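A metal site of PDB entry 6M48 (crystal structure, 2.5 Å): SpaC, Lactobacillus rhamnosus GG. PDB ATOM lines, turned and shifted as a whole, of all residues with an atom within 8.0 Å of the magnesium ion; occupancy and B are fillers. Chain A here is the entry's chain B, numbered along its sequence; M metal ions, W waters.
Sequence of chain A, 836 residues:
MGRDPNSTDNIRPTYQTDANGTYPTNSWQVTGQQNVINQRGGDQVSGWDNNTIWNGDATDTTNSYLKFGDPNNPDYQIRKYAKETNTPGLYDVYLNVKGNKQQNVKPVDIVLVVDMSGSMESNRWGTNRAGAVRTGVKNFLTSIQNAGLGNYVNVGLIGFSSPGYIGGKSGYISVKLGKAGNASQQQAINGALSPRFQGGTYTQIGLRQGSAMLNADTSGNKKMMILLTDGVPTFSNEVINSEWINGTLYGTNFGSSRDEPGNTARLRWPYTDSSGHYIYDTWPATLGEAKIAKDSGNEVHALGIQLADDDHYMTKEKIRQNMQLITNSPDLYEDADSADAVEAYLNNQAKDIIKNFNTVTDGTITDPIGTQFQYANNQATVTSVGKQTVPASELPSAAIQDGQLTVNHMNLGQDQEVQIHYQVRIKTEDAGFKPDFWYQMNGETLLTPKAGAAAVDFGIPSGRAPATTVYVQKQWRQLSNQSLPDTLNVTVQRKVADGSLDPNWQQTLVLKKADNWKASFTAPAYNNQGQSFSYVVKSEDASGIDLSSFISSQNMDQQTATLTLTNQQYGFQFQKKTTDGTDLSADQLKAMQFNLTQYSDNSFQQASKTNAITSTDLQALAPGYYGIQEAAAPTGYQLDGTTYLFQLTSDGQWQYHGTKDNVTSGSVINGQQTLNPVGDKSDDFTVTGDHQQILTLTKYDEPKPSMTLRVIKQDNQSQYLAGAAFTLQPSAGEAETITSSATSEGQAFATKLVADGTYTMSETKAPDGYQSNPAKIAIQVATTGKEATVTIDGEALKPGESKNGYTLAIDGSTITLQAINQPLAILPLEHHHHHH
Water W3 bridges the side-chain hydroxyl (OG1) of Thr 201 (2.4 Å) and the side-chain carboxylate (OD2) of Asp 115 (2.7 Å).
The magnesium ion is bound by the side-chain hydroxyl of Ser 119 (2.0 Å), the side-chain carboxylate of Asp 230 (2.1 Å), the side-chain hydroxyl of Ser 117 (2.1 Å), water W3 (2.1 Å), water W2 (2.1 Å) and water W1 (2.1 Å).
The backbone carbonyl oxygen of Ser 119 is in hydrogen-bond range of the side-chain amide nitrogen of Asn 123 (2.9 Å).
The backbone NH of Asp 230 sits at hydrogen-bond distance from the side-chain carboxylate of Asp 115, 3.3 Å away.
OD2 of Asp 230 sits at hydrogen-bond distance from N of Met 120 (3.3 Å).
The side-chain carboxylate (OD2) of Asp 230 is in salt-bridge range of the guanidinium group (NH1) of Arg 129 (2.9 Å).
The side-chain carboxylate of Asp 115 lies within hydrogen-bond range of the backbone NH of Ser 117 (2.9 Å).
The side-chain hydroxyl of Thr 229 lies within hydrogen-bond range of the side-chain carboxylate of Asp 115, at 2.5 Å.
The backbone NH of Thr 234 is in hydrogen-bond range of the backbone carbonyl oxygen of Thr 201 (2.9 Å).
Asp 115 touches the magnesium ion.
Thr 201 touches the magnesium ion (OG1 to MG, 3.98 Å).
Within 4 Å of the magnesium ion: Asp 115, Ser 117, Ser 119, Thr 201 and Asp 230.
The nearest printed residue that does not touch the magnesium ion is Gly 231 (4.5 Å).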
ATOM      1  N   ASP A 115     -27.535 -20.793   6.138  1.00  0.00           N
ATOM      2  CA  ASP A 115     -27.721 -22.240   5.867  1.00  0.00           C
ATOM      3  C   ASP A 115     -28.070 -22.943   7.194  1.00  0.00           C
ATOM      4  O   ASP A 115     -27.212 -23.073   8.074  1.00  0.00           O
ATOM      5  CB  ASP A 115     -26.422 -22.756   5.248  1.00  0.00           C
ATOM      6  CG  ASP A 115     -26.427 -24.220   4.891  1.00  0.00           C
ATOM      7  OD1 ASP A 115     -27.370 -24.921   5.415  1.00  0.00           O
ATOM      8  OD2 ASP A 115     -25.539 -24.646   4.051  1.00  0.00           O
ATOM      9  N   MET A 116     -29.340 -23.332   7.361  1.00  0.00           N
ATOM     10  CA  MET A 116     -29.839 -24.005   8.585  1.00  0.00           C
ATOM     11  C   MET A 116     -30.081 -25.481   8.260  1.00  0.00           C
ATOM     12  O   MET A 116     -30.977 -26.061   8.858  1.00  0.00           O
ATOM     13  CB  MET A 116     -31.104 -23.335   9.110  1.00  0.00           C
ATOM     14  CG  MET A 116     -30.837 -21.988   9.667  1.00  0.00           C
ATOM     15  SD  MET A 116     -32.340 -21.052   9.985  1.00  0.00           S
ATOM     16  CE  MET A 116     -32.805 -21.655  11.610  1.00  0.00           C
ATOM     17  N   SER A 117     -29.241 -26.048   7.395  1.00  0.00           N
ATOM     18  CA  SER A 117     -29.262 -27.478   6.961  1.00  0.00           C
ATOM     19  C   SER A 117     -28.914 -28.384   8.154  1.00  0.00           C
ATOM     20  O   SER A 117     -28.265 -27.891   9.070  1.00  0.00           O
ATOM     21  CB  SER A 117     -28.298 -27.712   5.795  1.00  0.00           C
ATOM     22  OG  SER A 117     -26.924 -27.625   6.228  1.00  0.00           O
ATOM     23  N   GLY A 118     -29.316 -29.665   8.134  1.00  0.00           N
ATOM     24  CA  GLY A 118     -29.094 -30.568   9.280  1.00  0.00           C
ATOM     25  C   GLY A 118     -27.626 -30.871   9.531  1.00  0.00           C
ATOM     26  O   GLY A 118     -27.266 -31.042  10.703  1.00  0.00           O
ATOM     27  N   SER A 119     -26.783 -30.890   8.484  1.00  0.00           N
ATOM     28  CA  SER A 119     -25.301 -31.059   8.587  1.00  0.00           C
ATOM     29  C   SER A 119     -24.712 -30.107   9.641  1.00  0.00           C
ATOM     30  O   SER A 119     -23.688 -30.457  10.236  1.00  0.00           O
ATOM     31  CB  SER A 119     -24.590 -30.867   7.274  1.00  0.00           C
ATOM     32  OG  SER A 119     -24.950 -29.616   6.718  1.00  0.00           O
ATOM     33  N   MET A 120     -25.303 -28.935   9.844  1.00  0.00           N
ATOM     34  CA  MET A 120     -24.725 -27.930  10.772  1.00  0.00           C
ATOM     35  C   MET A 120     -24.837 -28.482  12.189  1.00  0.00           C
ATOM     36  O   MET A 120     -24.144 -27.990  13.082  1.00  0.00           O
ATOM     37  CB  MET A 120     -25.472 -26.596  10.693  1.00  0.00           C
ATOM     38  CG  MET A 120     -25.409 -25.970   9.355  1.00  0.00           C
ATOM     39  SD  MET A 120     -23.882 -25.048   9.145  1.00  0.00           S
ATOM     40  CE  MET A 120     -24.260 -23.590  10.113  1.00  0.00           C
ATOM     41  N   GLU A 121     -25.701 -29.455  12.405  1.00  0.00           N
ATOM     42  CA  GLU A 121     -26.049 -29.975  13.762  1.00  0.00           C
ATOM     43  C   GLU A 121     -25.289 -31.300  14.003  1.00  0.00           C
ATOM     44  O   GLU A 121     -24.787 -31.527  15.106  1.00  0.00           O
ATOM     45  CB  GLU A 121     -27.584 -30.040  13.764  1.00  0.00           C
ATOM     46  CG  GLU A 121     -28.258 -29.689  15.061  1.00  0.00           C
ATOM     47  CD  GLU A 121     -28.235 -28.281  15.580  1.00  0.00           C
ATOM     48  OE1 GLU A 121     -29.063 -27.480  15.127  1.00  0.00           O
ATOM     49  OE2 GLU A 121     -27.457 -28.011  16.524  1.00  0.00           O
ATOM     50  N   SER A 122     -25.098 -32.102  12.959  1.00  0.00           N
ATOM     51  CA  SER A 122     -24.486 -33.450  13.002  1.00  0.00           C
ATOM     52  C   SER A 122     -23.622 -33.662  11.730  1.00  0.00           C
ATOM     53  O   SER A 122     -24.162 -33.640  10.591  1.00  0.00           O
ATOM     54  CB  SER A 122     -25.605 -34.466  13.163  1.00  0.00           C
ATOM     55  OG  SER A 122     -25.211 -35.781  12.780  1.00  0.00           O
ATOM     56  N   ASN A 123     -22.322 -33.876  11.883  1.00  0.00           N
ATOM     57  CA  ASN A 123     -21.441 -33.982  10.683  1.00  0.00           C
ATOM     58  C   ASN A 123     -20.213 -34.877  10.971  1.00  0.00           C
ATOM     59  O   ASN A 123     -20.000 -35.267  12.162  1.00  0.00           O
ATOM     60  CB  ASN A 123     -21.066 -32.567  10.233  1.00  0.00           C
ATOM     61  CG  ASN A 123     -20.485 -31.716  11.347  1.00  0.00           C
ATOM     62  OD1 ASN A 123     -19.364 -31.964  11.789  1.00  0.00           O
ATOM     63  ND2 ASN A 123     -21.200 -30.676  11.779  1.00  0.00           N
ATOM     64  N   ARG A 129     -21.459 -26.560  14.317  1.00  0.00           N
ATOM     65  CA  ARG A 129     -21.480 -25.411  13.381  1.00  0.00           C
ATOM     66  C   ARG A 129     -22.653 -24.484  13.760  1.00  0.00           C
ATOM     67  O   ARG A 129     -22.444 -23.273  13.874  1.00  0.00           O
ATOM     68  CB  ARG A 129     -21.644 -25.898  11.954  1.00  0.00           C
ATOM     69  CG  ARG A 129     -20.626 -26.938  11.575  1.00  0.00           C
ATOM     70  CD  ARG A 129     -20.738 -27.297  10.099  1.00  0.00           C
ATOM     71  NE  ARG A 129     -19.752 -28.318   9.809  1.00  0.00           N
ATOM     72  CZ  ARG A 129     -19.876 -29.302   8.912  1.00  0.00           C
ATOM     73  NH1 ARG A 129     -20.968 -29.428   8.180  1.00  0.00           N
ATOM     74  NH2 ARG A 129     -18.880 -30.162   8.749  1.00  0.00           N
ATOM     75  N   PHE A 160     -32.410 -20.451   5.750  1.00  0.00           N
ATOM     76  CA  PHE A 160     -32.911 -21.333   4.696  1.00  0.00           C
ATOM     77  C   PHE A 160     -32.486 -22.771   4.996  1.00  0.00           C
ATOM     78  O   PHE A 160     -31.491 -23.020   5.693  1.00  0.00           O
ATOM     79  CB  PHE A 160     -32.450 -20.808   3.353  1.00  0.00           C
ATOM     80  CG  PHE A 160     -31.004 -21.037   3.087  1.00  0.00           C
ATOM     81  CD1 PHE A 160     -30.569 -22.248   2.547  1.00  0.00           C
ATOM     82  CD2 PHE A 160     -30.081 -20.026   3.313  1.00  0.00           C
ATOM     83  CE1 PHE A 160     -29.226 -22.436   2.266  1.00  0.00           C
ATOM     84  CE2 PHE A 160     -28.744 -20.213   3.020  1.00  0.00           C
ATOM     85  CZ  PHE A 160     -28.311 -21.426   2.529  1.00  0.00           C
ATOM     86  N   GLY A 199     -32.570 -29.989   7.459  1.00  0.00           N
ATOM     87  CA  GLY A 199     -33.004 -29.942   6.069  1.00  0.00           C
ATOM     88  C   GLY A 199     -31.848 -29.870   5.083  1.00  0.00           C
ATOM     89  O   GLY A 199     -30.677 -29.994   5.524  1.00  0.00           O
ATOM     90  N   GLY A 200     -32.202 -29.678   3.814  1.00  0.00           N
ATOM     91  CA  GLY A 200     -31.276 -29.541   2.680  1.00  0.00           C
ATOM     92  C   GLY A 200     -30.809 -28.106   2.560  1.00  0.00           C
ATOM     93  O   GLY A 200     -30.882 -27.362   3.595  1.00  0.00           O
ATOM     94  N   THR A 201     -30.328 -27.740   1.362  1.00  0.00           N
ATOM     95  CA  THR A 201     -29.581 -26.480   1.092  1.00  0.00           C
ATOM     96  C   THR A 201     -30.171 -25.772  -0.152  1.00  0.00           C
ATOM     97  O   THR A 201     -29.668 -25.979  -1.262  1.00  0.00           O
ATOM     98  CB  THR A 201     -28.074 -26.761   0.982  1.00  0.00           C
ATOM     99  OG1 THR A 201     -27.698 -27.711   1.990  1.00  0.00           O
ATOM    100  CG2 THR A 201     -27.254 -25.503   1.137  1.00  0.00           C
ATOM    101  N   THR A 229     -22.563 -20.937   5.035  1.00  0.00           N
ATOM    102  CA  THR A 229     -23.009 -22.216   4.464  1.00  0.00           C
ATOM    103  C   THR A 229     -21.943 -23.290   4.686  1.00  0.00           C
ATOM    104  O   THR A 229     -20.797 -22.949   4.674  1.00  0.00           O
ATOM    105  CB  THR A 229     -23.382 -22.012   2.998  1.00  0.00           C
ATOM    106  OG1 THR A 229     -24.023 -23.220   2.580  1.00  0.00           O
ATOM    107  CG2 THR A 229     -22.182 -21.695   2.144  1.00  0.00           C
ATOM    108  N   ASP A 230     -22.360 -24.539   4.867  1.00  0.00           N
ATOM    109  CA  ASP A 230     -21.517 -25.710   5.172  1.00  0.00           C
ATOM    110  C   ASP A 230     -21.699 -26.773   4.068  1.00  0.00           C
ATOM    111  O   ASP A 230     -21.461 -28.005   4.360  1.00  0.00           O
ATOM    112  CB  ASP A 230     -21.860 -26.260   6.557  1.00  0.00           C
ATOM    113  CG  ASP A 230     -23.132 -27.103   6.546  1.00  0.00           C
ATOM    114  OD1 ASP A 230     -23.944 -26.955   5.596  1.00  0.00           O
ATOM    115  OD2 ASP A 230     -23.324 -27.842   7.504  1.00  0.00           O
ATOM    116  N   GLY A 231     -22.086 -26.350   2.850  1.00  0.00           N
ATOM    117  CA  GLY A 231     -22.521 -27.305   1.820  1.00  0.00           C
ATOM    118  C   GLY A 231     -22.722 -26.727   0.446  1.00  0.00           C
ATOM    119  O   GLY A 231     -22.963 -25.544   0.295  1.00  0.00           O
ATOM    120  N   VAL A 232     -22.649 -27.566  -0.548  1.00  0.00           N
ATOM    121  CA  VAL A 232     -23.104 -27.202  -1.896  1.00  0.00           C
ATOM    122  C   VAL A 232     -24.617 -27.063  -1.834  1.00  0.00           C
ATOM    123  O   VAL A 232     -25.312 -27.605  -0.946  1.00  0.00           O
ATOM    124  CB  VAL A 232     -22.674 -28.278  -2.916  1.00  0.00           C
ATOM    125  CG1 VAL A 232     -21.145 -28.450  -2.925  1.00  0.00           C
ATOM    126  CG2 VAL A 232     -23.429 -29.609  -2.728  1.00  0.00           C
ATOM    127  N   THR A 234     -28.286 -27.966  -2.770  1.00  0.00           N
ATOM    128  CA  THR A 234     -28.958 -29.224  -3.192  1.00  0.00           C
ATOM    129  C   THR A 234     -30.389 -28.952  -3.656  1.00  0.00           C
ATOM    130  O   THR A 234     -31.050 -29.881  -4.073  1.00  0.00           O
ATOM    131  CB  THR A 234     -28.848 -30.248  -2.061  1.00  0.00           C
ATOM    132  OG1 THR A 234     -29.468 -29.690  -0.903  1.00  0.00           O
ATOM    133  CG2 THR A 234     -27.407 -30.625  -1.794  1.00  0.00           C
ATOM    134  N   ILE A 305     -18.038 -23.301   5.590  1.00  0.00           N
ATOM    135  CA  ILE A 305     -17.711 -23.974   6.875  1.00  0.00           C
ATOM    136  C   ILE A 305     -17.387 -25.441   6.596  1.00  0.00           C
ATOM    137  O   ILE A 305     -18.305 -26.220   6.234  1.00  0.00           O
ATOM    138  CB  ILE A 305     -18.890 -23.823   7.842  1.00  0.00           C
ATOM    139  CG1 ILE A 305     -19.369 -22.379   7.937  1.00  0.00           C
ATOM    140  CG2 ILE A 305     -18.546 -24.385   9.216  1.00  0.00           C
ATOM    141  CD1 ILE A 305     -20.580 -22.228   8.825  1.00  0.00           C
HETATM  142 MG    MG M   1     -25.340 -28.415   5.116  1.00  0.00          MG
HETATM  143  O   HOH W   1     -26.261 -30.150   4.323  1.00  0.00           O
HETATM  144  O   HOH W   2     -23.786 -29.540   4.247  1.00  0.00           O
HETATM  145  O   HOH W   3     -25.800 -27.258   3.434  1.00  0.00           O
